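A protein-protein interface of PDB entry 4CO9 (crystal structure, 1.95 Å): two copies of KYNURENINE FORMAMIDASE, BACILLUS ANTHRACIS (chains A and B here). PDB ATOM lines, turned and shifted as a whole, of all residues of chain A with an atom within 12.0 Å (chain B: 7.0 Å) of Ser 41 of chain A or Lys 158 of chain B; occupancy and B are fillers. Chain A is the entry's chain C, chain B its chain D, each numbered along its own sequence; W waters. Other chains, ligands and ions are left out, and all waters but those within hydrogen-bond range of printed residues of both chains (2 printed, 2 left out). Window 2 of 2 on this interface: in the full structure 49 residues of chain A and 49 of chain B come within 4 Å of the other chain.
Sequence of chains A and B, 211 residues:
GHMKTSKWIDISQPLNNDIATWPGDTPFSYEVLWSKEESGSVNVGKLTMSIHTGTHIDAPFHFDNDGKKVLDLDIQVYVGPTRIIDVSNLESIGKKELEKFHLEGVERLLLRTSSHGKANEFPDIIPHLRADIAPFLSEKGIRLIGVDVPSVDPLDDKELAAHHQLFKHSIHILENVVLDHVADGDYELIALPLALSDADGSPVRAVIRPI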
ATOM      1  N   TYR A  30      -2.809 -24.007  13.715  1.00  0.00           N
ATOM      2  CA  TYR A  30      -2.808 -23.177  12.515  1.00  0.00           C
ATOM      3  C   TYR A  30      -4.239 -23.068  12.006  1.00  0.00           C
ATOM      4  O   TYR A  30      -4.907 -24.084  11.822  1.00  0.00           O
ATOM      5  CB  TYR A  30      -1.897 -23.701  11.384  1.00  0.00           C
ATOM      6  CG  TYR A  30      -2.114 -22.846  10.155  1.00  0.00           C
ATOM      7  CD1 TYR A  30      -1.443 -21.644   9.987  1.00  0.00           C
ATOM      8  CD2 TYR A  30      -3.069 -23.185   9.213  1.00  0.00           C
ATOM      9  CE1 TYR A  30      -1.682 -20.810   8.903  1.00  0.00           C
ATOM     10  CE2 TYR A  30      -3.323 -22.357   8.132  1.00  0.00           C
ATOM     11  CZ  TYR A  30      -2.637 -21.178   7.970  1.00  0.00           C
ATOM     12  OH  TYR A  30      -2.920 -20.380   6.873  1.00  0.00           O
ATOM     13  N   VAL A  32      -6.880 -20.669   9.170  1.00  0.00           N
ATOM     14  CA  VAL A  32      -7.192 -19.604   8.230  1.00  0.00           C
ATOM     15  C   VAL A  32      -8.285 -18.755   8.876  1.00  0.00           C
ATOM     16  O   VAL A  32      -9.429 -19.202   9.033  1.00  0.00           O
ATOM     17  CB  VAL A  32      -7.691 -20.138   6.869  1.00  0.00           C
ATOM     18  CG1 VAL A  32      -7.987 -18.995   5.902  1.00  0.00           C
ATOM     19  CG2 VAL A  32      -6.666 -21.075   6.267  1.00  0.00           C
ATOM     20  N   LEU A  33      -7.919 -17.565   9.314  1.00  0.00           N
ATOM     21  CA  LEU A  33      -8.881 -16.650   9.942  1.00  0.00           C
ATOM     22  C   LEU A  33      -9.852 -16.066   8.936  1.00  0.00           C
ATOM     23  O   LEU A  33     -11.018 -15.842   9.236  1.00  0.00           O
ATOM     24  CB  LEU A  33      -8.192 -15.470  10.598  1.00  0.00           C
ATOM     25  CG  LEU A  33      -7.329 -15.689  11.836  1.00  0.00           C
ATOM     26  CD1 LEU A  33      -6.769 -14.386  12.400  1.00  0.00           C
ATOM     27  CD2 LEU A  33      -8.126 -16.426  12.891  1.00  0.00           C
ATOM     28  N   TRP A  34      -9.313 -15.702   7.783  1.00  0.00           N
ATOM     29  CA  TRP A  34     -10.061 -14.956   6.789  1.00  0.00           C
ATOM     30  C   TRP A  34      -9.586 -15.457   5.430  1.00  0.00           C
ATOM     31  O   TRP A  34      -8.423 -15.309   5.089  1.00  0.00           O
ATOM     32  CB  TRP A  34      -9.721 -13.487   7.049  1.00  0.00           C
ATOM     33  CG  TRP A  34     -10.651 -12.423   6.487  1.00  0.00           C
ATOM     34  CD1 TRP A  34     -10.294 -11.327   5.717  1.00  0.00           C
ATOM     35  CD2 TRP A  34     -12.075 -12.334   6.662  1.00  0.00           C
ATOM     36  NE1 TRP A  34     -11.411 -10.593   5.405  1.00  0.00           N
ATOM     37  CE2 TRP A  34     -12.512 -11.179   5.967  1.00  0.00           C
ATOM     38  CE3 TRP A  34     -13.023 -13.115   7.334  1.00  0.00           C
ATOM     39  CZ2 TRP A  34     -13.859 -10.792   5.926  1.00  0.00           C
ATOM     40  CZ3 TRP A  34     -14.369 -12.737   7.279  1.00  0.00           C
ATOM     41  CH2 TRP A  34     -14.767 -11.583   6.580  1.00  0.00           C
ATOM     42  N   SER A  35     -10.496 -16.105   4.706  1.00  0.00           N
ATOM     43  CA  SER A  35     -10.192 -16.823   3.469  1.00  0.00           C
ATOM     44  C   SER A  35     -10.009 -15.857   2.304  1.00  0.00           C
ATOM     45  O   SER A  35     -10.432 -14.703   2.376  1.00  0.00           O
ATOM     46  CB  SER A  35     -11.338 -17.767   3.148  1.00  0.00           C
ATOM     47  OG  SER A  35     -12.493 -17.049   2.763  1.00  0.00           O
ATOM     48  N   LYS A  36      -9.419 -16.338   1.220  1.00  0.00           N
ATOM     49  CA  LYS A  36      -9.335 -15.553  -0.006  1.00  0.00           C
ATOM     50  C   LYS A  36     -10.726 -15.141  -0.521  1.00  0.00           C
ATOM     51  O   LYS A  36     -10.895 -14.039  -1.050  1.00  0.00           O
ATOM     52  CB  LYS A  36      -8.569 -16.328  -1.085  1.00  0.00           C
ATOM     53  CG  LYS A  36      -8.509 -15.619  -2.424  1.00  0.00           C
ATOM     54  CD  LYS A  36      -7.537 -16.275  -3.390  1.00  0.00           C
ATOM     55  CE  LYS A  36      -7.516 -15.489  -4.684  1.00  0.00           C
ATOM     56  NZ  LYS A  36      -6.522 -16.019  -5.644  1.00  0.00           N
ATOM     57  N   GLU A  37     -11.710 -16.024  -0.379  1.00  0.00           N
ATOM     58  CA  GLU A  37     -13.095 -15.708  -0.766  1.00  0.00           C
ATOM     59  C   GLU A  37     -13.640 -14.547   0.056  1.00  0.00           C
ATOM     60  O   GLU A  37     -14.233 -13.624  -0.489  1.00  0.00           O
ATOM     61  CB  GLU A  37     -13.981 -16.925  -0.574  1.00  0.00           C
ATOM     62  CG  GLU A  37     -15.341 -16.855  -1.215  1.00  0.00           C
ATOM     63  CD  GLU A  37     -16.258 -17.980  -0.754  1.00  0.00           C
ATOM     64  OE1 GLU A  37     -15.759 -19.007  -0.231  1.00  0.00           O
ATOM     65  OE2 GLU A  37     -17.491 -17.849  -0.917  1.00  0.00           O
ATOM     66  N   GLU A  38     -13.385 -14.578   1.358  1.00  0.00           N
ATOM     67  CA  GLU A  38     -13.795 -13.492   2.260  1.00  0.00           C
ATOM     68  C   GLU A  38     -13.026 -12.180   2.052  1.00  0.00           C
ATOM     69  O   GLU A  38     -13.639 -11.111   2.010  1.00  0.00           O
ATOM     70  CB  GLU A  38     -13.713 -13.945   3.728  1.00  0.00           C
ATOM     71  CG  GLU A  38     -14.703 -15.099   4.047  1.00  0.00           C
ATOM     72  CD  GLU A  38     -14.424 -15.838   5.321  1.00  0.00           C
ATOM     73  OE1 GLU A  38     -13.260 -15.936   5.771  1.00  0.00           O
ATOM     74  OE2 GLU A  38     -15.424 -16.344   5.859  1.00  0.00           O
ATOM     75  N   SER A  39     -11.708 -12.257   1.937  1.00  0.00           N
ATOM     76  CA  SER A  39     -10.870 -11.067   1.843  1.00  0.00           C
ATOM     77  C   SER A  39     -10.873 -10.458   0.438  1.00  0.00           C
ATOM     78  O   SER A  39     -10.555  -9.294   0.276  1.00  0.00           O
ATOM     79  CB  SER A  39      -9.414 -11.392   2.217  1.00  0.00           C
ATOM     80  OG  SER A  39      -8.783 -12.198   1.231  1.00  0.00           O
ATOM     81  N   GLY A  40     -11.129 -11.288  -0.568  1.00  0.00           N
ATOM     82  CA  GLY A  40     -10.991 -10.883  -1.949  1.00  0.00           C
ATOM     83  C   GLY A  40      -9.574 -10.944  -2.494  1.00  0.00           C
ATOM     84  O   GLY A  40      -9.334 -10.495  -3.603  1.00  0.00           O
ATOM     85  N   SER A  41      -8.607 -11.484  -1.750  1.00  0.00           N
ATOM     86  CA  SER A  41      -7.258 -11.597  -2.301  1.00  0.00           C
ATOM     87  C   SER A  41      -6.385 -12.680  -1.699  1.00  0.00           C
ATOM     88  O   SER A  41      -5.673 -13.357  -2.431  1.00  0.00           O
ATOM     89  CB  SER A  41      -6.505 -10.258  -2.288  1.00  0.00           C
ATOM     90  OG  SER A  41      -6.214  -9.835  -0.998  1.00  0.00           O
ATOM     91  N   VAL A  42      -6.435 -12.842  -0.377  1.00  0.00           N
ATOM     92  CA  VAL A  42      -5.492 -13.706   0.327  1.00  0.00           C
ATOM     93  C   VAL A  42      -6.141 -14.557   1.424  1.00  0.00           C
ATOM     94  O   VAL A  42      -7.188 -14.203   2.006  1.00  0.00           O
ATOM     95  CB  VAL A  42      -4.376 -12.870   0.985  1.00  0.00           C
ATOM     96  CG1 VAL A  42      -3.481 -12.279  -0.080  1.00  0.00           C
ATOM     97  CG2 VAL A  42      -4.968 -11.759   1.873  1.00  0.00           C
ATOM     98  N   ASN A  43      -5.522 -15.704   1.669  1.00  0.00           N
ATOM     99  CA  ASN A  43      -5.793 -16.498   2.851  1.00  0.00           C
ATOM    100  C   ASN A  43      -4.952 -15.965   4.004  1.00  0.00           C
ATOM    101  O   ASN A  43      -3.749 -15.939   3.914  1.00  0.00           O
ATOM    102  CB  ASN A  43      -5.496 -17.966   2.557  1.00  0.00           C
ATOM    103  CG  ASN A  43      -6.480 -18.554   1.563  1.00  0.00           C
ATOM    104  OD1 ASN A  43      -7.685 -18.538   1.809  1.00  0.00           O
ATOM    105  ND2 ASN A  43      -5.988 -19.012   0.426  1.00  0.00           N
ATOM    106  N   VAL A  44      -5.620 -15.516   5.063  1.00  0.00           N
ATOM    107  CA  VAL A  44      -4.948 -14.892   6.191  1.00  0.00           C
ATOM    108  C   VAL A  44      -4.981 -15.866   7.346  1.00  0.00           C
ATOM    109  O   VAL A  44      -6.052 -16.221   7.853  1.00  0.00           O
ATOM    110  CB  VAL A  44      -5.617 -13.564   6.562  1.00  0.00           C
ATOM    111  CG1 VAL A  44      -4.973 -12.967   7.813  1.00  0.00           C
ATOM    112  CG2 VAL A  44      -5.487 -12.607   5.380  1.00  0.00           C
ATOM    113  N   GLY A  45      -3.793 -16.238   7.788  1.00  0.00           N
ATOM    114  CA  GLY A  45      -3.605 -17.330   8.708  1.00  0.00           C
ATOM    115  C   GLY A  45      -3.239 -16.807  10.076  1.00  0.00           C
ATOM    116  O   GLY A  45      -2.867 -15.631  10.238  1.00  0.00           O
ATOM    117  N   TRP B  22       1.227  -6.452   8.922  1.00  0.00           N
ATOM    118  CA  TRP B  22       0.273  -5.934   7.958  1.00  0.00           C
ATOM    119  C   TRP B  22      -0.943  -5.403   8.639  1.00  0.00           C
ATOM    120  O   TRP B  22      -1.340  -5.895   9.710  1.00  0.00           O
ATOM    121  CB  TRP B  22      -0.234  -7.003   7.006  1.00  0.00           C
ATOM    122  CG  TRP B  22       0.670  -7.275   5.949  1.00  0.00           C
ATOM    123  CD1 TRP B  22       1.781  -8.052   6.020  1.00  0.00           C
ATOM    124  CD2 TRP B  22       0.609  -6.752   4.613  1.00  0.00           C
ATOM    125  NE1 TRP B  22       2.415  -8.064   4.798  1.00  0.00           N
ATOM    126  CE2 TRP B  22       1.720  -7.260   3.925  1.00  0.00           C
ATOM    127  CE3 TRP B  22      -0.278  -5.905   3.935  1.00  0.00           C
ATOM    128  CZ2 TRP B  22       1.962  -6.961   2.586  1.00  0.00           C
ATOM    129  CZ3 TRP B  22      -0.030  -5.601   2.606  1.00  0.00           C
ATOM    130  CH2 TRP B  22       1.082  -6.123   1.947  1.00  0.00           C
ATOM    131  N   PHE B  61      -0.325 -21.031  -1.372  1.00  0.00           N
ATOM    132  CA  PHE B  61      -1.640 -21.048  -0.729  1.00  0.00           C
ATOM    133  C   PHE B  61      -2.055 -19.679  -0.194  1.00  0.00           C
ATOM    134  O   PHE B  61      -3.252 -19.383  -0.095  1.00  0.00           O
ATOM    135  CB  PHE B  61      -1.675 -22.084   0.385  1.00  0.00           C
ATOM    136  CG  PHE B  61      -2.956 -22.112   1.151  1.00  0.00           C
ATOM    137  CD1 PHE B  61      -4.168 -22.345   0.506  1.00  0.00           C
ATOM    138  CD2 PHE B  61      -2.964 -21.928   2.523  1.00  0.00           C
ATOM    139  CE1 PHE B  61      -5.349 -22.377   1.219  1.00  0.00           C
ATOM    140  CE2 PHE B  61      -4.154 -21.941   3.241  1.00  0.00           C
ATOM    141  CZ  PHE B  61      -5.341 -22.179   2.596  1.00  0.00           C
ATOM    142  N   HIS B  62      -1.076 -18.840   0.130  1.00  0.00           N
ATOM    143  CA  HIS B  62      -1.356 -17.474   0.570  1.00  0.00           C
ATOM    144  C   HIS B  62      -2.242 -16.704  -0.416  1.00  0.00           C
ATOM    145  O   HIS B  62      -3.134 -15.968  -0.005  1.00  0.00           O
ATOM    146  CB  HIS B  62      -0.039 -16.716   0.793  1.00  0.00           C
ATOM    147  CG  HIS B  62      -0.220 -15.283   1.176  1.00  0.00           C
ATOM    148  ND1 HIS B  62      -1.052 -14.882   2.194  1.00  0.00           N
ATOM    149  CD2 HIS B  62       0.343 -14.154   0.680  1.00  0.00           C
ATOM    150  CE1 HIS B  62      -1.008 -13.565   2.309  1.00  0.00           C
ATOM    151  NE2 HIS B  62      -0.179 -13.102   1.396  1.00  0.00           N
ATOM    152  N   PHE B  63      -1.971 -16.850  -1.706  1.00  0.00           N
ATOM    153  CA  PHE B  63      -2.666 -16.068  -2.725  1.00  0.00           C
ATOM    154  C   PHE B  63      -3.432 -16.913  -3.742  1.00  0.00           C
ATOM    155  O   PHE B  63      -4.082 -16.363  -4.634  1.00  0.00           O
ATOM    156  CB  PHE B  63      -1.686 -15.134  -3.442  1.00  0.00           C
ATOM    157  CG  PHE B  63      -0.442 -15.819  -3.919  1.00  0.00           C
ATOM    158  CD1 PHE B  63      -0.416 -16.435  -5.158  1.00  0.00           C
ATOM    159  CD2 PHE B  63       0.696 -15.843  -3.133  1.00  0.00           C
ATOM    160  CE1 PHE B  63       0.727 -17.066  -5.613  1.00  0.00           C
ATOM    161  CE2 PHE B  63       1.853 -16.465  -3.590  1.00  0.00           C
ATOM    162  CZ  PHE B  63       1.860 -17.081  -4.837  1.00  0.00           C
ATOM    163  N   ASP B  64      -3.387 -18.231  -3.585  1.00  0.00           N
ATOM    164  CA  ASP B  64      -4.067 -19.144  -4.482  1.00  0.00           C
ATOM    165  C   ASP B  64      -4.625 -20.287  -3.665  1.00  0.00           C
ATOM    166  O   ASP B  64      -3.868 -21.059  -3.065  1.00  0.00           O
ATOM    167  CB  ASP B  64      -3.085 -19.658  -5.531  1.00  0.00           C
ATOM    168  CG  ASP B  64      -3.749 -20.524  -6.603  1.00  0.00           C
ATOM    169  OD1 ASP B  64      -4.737 -21.230  -6.335  1.00  0.00           O
ATOM    170  OD2 ASP B  64      -3.249 -20.497  -7.745  1.00  0.00           O
ATOM    171  N   PRO B 154       2.590  -3.984  -4.715  1.00  0.00           N
ATOM    172  CA  PRO B 154       2.240  -2.782  -3.971  1.00  0.00           C
ATOM    173  C   PRO B 154       1.366  -3.100  -2.762  1.00  0.00           C
ATOM    174  O   PRO B 154       0.565  -4.035  -2.793  1.00  0.00           O
ATOM    175  CB  PRO B 154       1.464  -1.937  -4.994  1.00  0.00           C
ATOM    176  CG  PRO B 154       1.890  -2.446  -6.322  1.00  0.00           C
ATOM    177  CD  PRO B 154       2.109  -3.921  -6.108  1.00  0.00           C
ATOM    178  N   LEU B 155       1.520  -2.318  -1.708  1.00  0.00           N
ATOM    179  CA  LEU B 155       0.851  -2.609  -0.443  1.00  0.00           C
ATOM    180  C   LEU B 155      -0.671  -2.572  -0.535  1.00  0.00           C
ATOM    181  O   LEU B 155      -1.354  -3.287   0.199  1.00  0.00           O
ATOM    182  CB  LEU B 155       1.311  -1.632   0.633  1.00  0.00           C
ATOM    183  CG  LEU B 155       2.807  -1.636   0.937  1.00  0.00           C
ATOM    184  CD1 LEU B 155       3.097  -0.567   1.979  1.00  0.00           C
ATOM    185  CD2 LEU B 155       3.294  -3.005   1.398  1.00  0.00           C
ATOM    186  N   ASP B 156      -1.197  -1.746  -1.431  1.00  0.00           N
ATOM    187  CA  ASP B 156      -2.648  -1.602  -1.571  1.00  0.00           C
ATOM    188  C   ASP B 156      -3.230  -2.486  -2.673  1.00  0.00           C
ATOM    189  O   ASP B 156      -4.431  -2.455  -2.904  1.00  0.00           O
ATOM    190  CB  ASP B 156      -3.022  -0.132  -1.822  1.00  0.00           C
ATOM    191  CG  ASP B 156      -2.454   0.415  -3.138  1.00  0.00           C
ATOM    192  OD1 ASP B 156      -1.622  -0.259  -3.787  1.00  0.00           O
ATOM    193  OD2 ASP B 156      -2.813   1.547  -3.515  1.00  0.00           O
ATOM    194  N   ASP B 157      -2.390  -3.283  -3.334  1.00  0.00           N
ATOM    195  CA  ASP B 157      -2.812  -4.086  -4.472  1.00  0.00           C
ATOM    196  C   ASP B 157      -3.507  -5.371  -4.027  1.00  0.00           C
ATOM    197  O   ASP B 157      -2.956  -6.154  -3.241  1.00  0.00           O
ATOM    198  CB  ASP B 157      -1.609  -4.439  -5.350  1.00  0.00           C
ATOM    199  CG  ASP B 157      -1.994  -5.268  -6.551  1.00  0.00           C
ATOM    200  OD1 ASP B 157      -3.057  -5.016  -7.137  1.00  0.00           O
ATOM    201  OD2 ASP B 157      -1.249  -6.192  -6.909  1.00  0.00           O
ATOM    202  N   LYS B 158      -4.712  -5.598  -4.533  1.00  0.00           N
ATOM    203  CA  LYS B 158      -5.465  -6.804  -4.198  1.00  0.00           C
ATOM    204  C   LYS B 158      -5.305  -7.920  -5.225  1.00  0.00           C
ATOM    205  O   LYS B 158      -5.701  -9.047  -4.969  1.00  0.00           O
ATOM    206  CB  LYS B 158      -6.954  -6.480  -4.047  1.00  0.00           C
ATOM    207  CG  LYS B 158      -7.257  -5.418  -3.010  1.00  0.00           C
ATOM    208  CD  LYS B 158      -6.723  -5.799  -1.641  1.00  0.00           C
ATOM    209  CE  LYS B 158      -7.263  -4.885  -0.564  1.00  0.00           C
ATOM    210  NZ  LYS B 158      -6.483  -5.016   0.699  1.00  0.00           N
ATOM    211  N   GLU B 159      -4.747  -7.619  -6.389  1.00  0.00           N
ATOM    212  CA  GLU B 159      -4.571  -8.624  -7.436  1.00  0.00           C
ATOM    213  C   GLU B 159      -3.291  -9.444  -7.233  1.00  0.00           C
ATOM    214  O   GLU B 159      -3.224 -10.608  -7.617  1.00  0.00           O
ATOM    215  CB  GLU B 159      -4.589  -7.945  -8.815  1.00  0.00           C
ATOM    216  CG  GLU B 159      -5.872  -7.153  -9.108  1.00  0.00           C
ATOM    217  CD  GLU B 159      -7.144  -7.892  -8.707  1.00  0.00           C
ATOM    218  OE1 GLU B 159      -7.356  -9.026  -9.181  1.00  0.00           O
ATOM    219  OE2 GLU B 159      -7.940  -7.344  -7.924  1.00  0.00           O
ATOM    220  N   LEU B 160      -2.275  -8.822  -6.647  1.00  0.00           N
ATOM    221  CA  LEU B 160      -0.999  -9.477  -6.376  1.00  0.00           C
ATOM    222  C   LEU B 160      -0.409 -10.114  -7.629  1.00  0.00           C
ATOM    223  O   LEU B 160      -0.068 -11.302  -7.647  1.00  0.00           O
ATOM    224  CB  LEU B 160      -1.150 -10.514  -5.268  1.00  0.00           C
ATOM    225  CG  LEU B 160      -1.641 -10.010  -3.912  1.00  0.00           C
ATOM    226  CD1 LEU B 160      -1.485 -11.119  -2.900  1.00  0.00           C
ATOM    227  CD2 LEU B 160      -0.896  -8.759  -3.469  1.00  0.00           C
ATOM    228  N   ALA B 161      -0.267  -9.303  -8.675  1.00  0.00           N
ATOM    229  CA  ALA B 161       0.237  -9.783  -9.957  1.00  0.00           C
ATOM    230  C   ALA B 161       1.640 -10.364  -9.837  1.00  0.00           C
ATOM    231  O   ALA B 161       1.937 -11.402 -10.434  1.00  0.00           O
ATOM    232  CB  ALA B 161       0.215  -8.666 -11.000  1.00  0.00           C
ATOM    233  N   HIS B 164       1.584 -13.884  -8.124  1.00  0.00           N
ATOM    234  CA  HIS B 164       1.037 -14.853  -9.053  1.00  0.00           C
ATOM    235  C   HIS B 164       2.000 -15.179 -10.187  1.00  0.00           C
ATOM    236  O   HIS B 164       2.230 -16.340 -10.474  1.00  0.00           O
ATOM    237  CB  HIS B 164      -0.286 -14.363  -9.627  1.00  0.00           C
ATOM    238  CG  HIS B 164      -1.446 -14.588  -8.713  1.00  0.00           C
ATOM    239  ND1 HIS B 164      -1.909 -13.625  -7.841  1.00  0.00           N
ATOM    240  CD2 HIS B 164      -2.210 -15.682  -8.503  1.00  0.00           C
ATOM    241  CE1 HIS B 164      -2.919 -14.115  -7.144  1.00  0.00           C
ATOM    242  NE2 HIS B 164      -3.118 -15.362  -7.528  1.00  0.00           N
HETATM  243  O   HOH W   1      -4.744 -13.222  -5.044  1.00  0.00           O
HETATM  244  O   HOH W   2      -5.396 -17.991  -7.983  1.00  0.00           O
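Water W1 lies within hydrogen-bond range of O of Ser 41 of chain A (2.8 Å), O of Phe 63 of chain B (3.2 Å) and NZ of Lys 36 of chain A (3.4 Å).
Water W2 bridges the side-chain amino group (NZ) of Lys 36 of chain A (3.3 Å) and the side-chain carboxylate (OD2) of Asp 64 of chain B (3.3 Å).
The backbone NH (N) of Lys 36 of chain A is in hydrogen-bond range of the side-chain amide oxygen (OD1) of Asn 43 of chain A (2.9 Å).
N of Ser 41 of chain A lies within hydrogen-bond range of OG of Ser 39 of chain A (3.1 Å).
The side-chain hydroxyl of Ser 39 of chain A lies within hydrogen-bond range of the backbone carbonyl oxygen of Val 42 of chain A (2.7 Å).
OD2 of Asp 157 of chain B is in hydrogen-bond range of N of Leu 160 of chain B, 2.8 Å away.
A ring nitrogen (ND1) of His 164 of chain B is in hydrogen-bond range of the backbone carbonyl oxygen (O) of Glu 159 of chain B.
The backbone carbonyl oxygen (O) of Leu 160 of chain B sits at hydrogen-bond distance from a ring nitrogen (ND1) of His 164 of chain B, at 3.0 Å.
Of the 14 printed residues of chain B, 6 touch a printed residue of chain A.
Printed residues of chain A that touch a printed residue of chain B: Lys 36, Ser 41, Val 42 and Asn 43.
Hydrophobic or aromatic side chains of chain A that line the printed part of chain B: Val 42.
Along chain A the printed residues that touch a printed residue of chain B span positions 36 to 43.
Among the printed residues, 7 pairs touch across the chains.
Ser 41 of chain A touches just one residue of chain B: Lys 158.
Lys 158 of chain B touches one residue of chain A.
His 62 of chain B touches two residues of chain A.
Pro 154 of chain B touches none of the printed residues of chain A.
Asp 156 of chain B touches none of the printed residues of chain A.
No residue of chain A comes within 4 Å of Asp 157 of chain B.
No residue of chain A comes within 4 Å of Glu 159 of chain B.
Of the printed residues of chain A, His 164 of chain B touches Lys 36.
Of the printed residues of chain B, Lys 36 of chain A touches Phe 63 and His 164.
Of the printed residues of chain A, Phe 61 of chain B touches Asn 43 (2.8 Å).
The nearest residue of chain B that does not touch Ser 41 of chain A is Phe 63 of chain B (4.1 Å).
The nearest printed residue of chain B that does not touch Asn 43 of chain A is Asp 64 of chain B (4.5 Å).
Lys 36 of chain A touches His 164 of chain B.
Lys 158 of chain B touches Ser 41 of chain A.
O of His 62 of chain B touches CA of Val 42 of chain A, at 3.3 Å.
Val 42 of chain A touches Leu 160 of chain B (CG1 to CD1, 3.6 Å).
No position is printed for both chains.
Of the 7 pairs that touch across the chains among the printed residues, none has its exchanged pair printed and touching as well.
The side-chain amino group (NZ) of Lys 36 of chain A sits at hydrogen-bond distance from the backbone carbonyl oxygen (O) of Phe 63 of chain B (2.7 Å).
ND2 of Asn 43 of chain A sits at hydrogen-bond distance from O of Phe 61 of chain B, at 2.8 Å.
N of Asn 43 of chain A sits at hydrogen-bond distance from O of His 62 of chain B.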
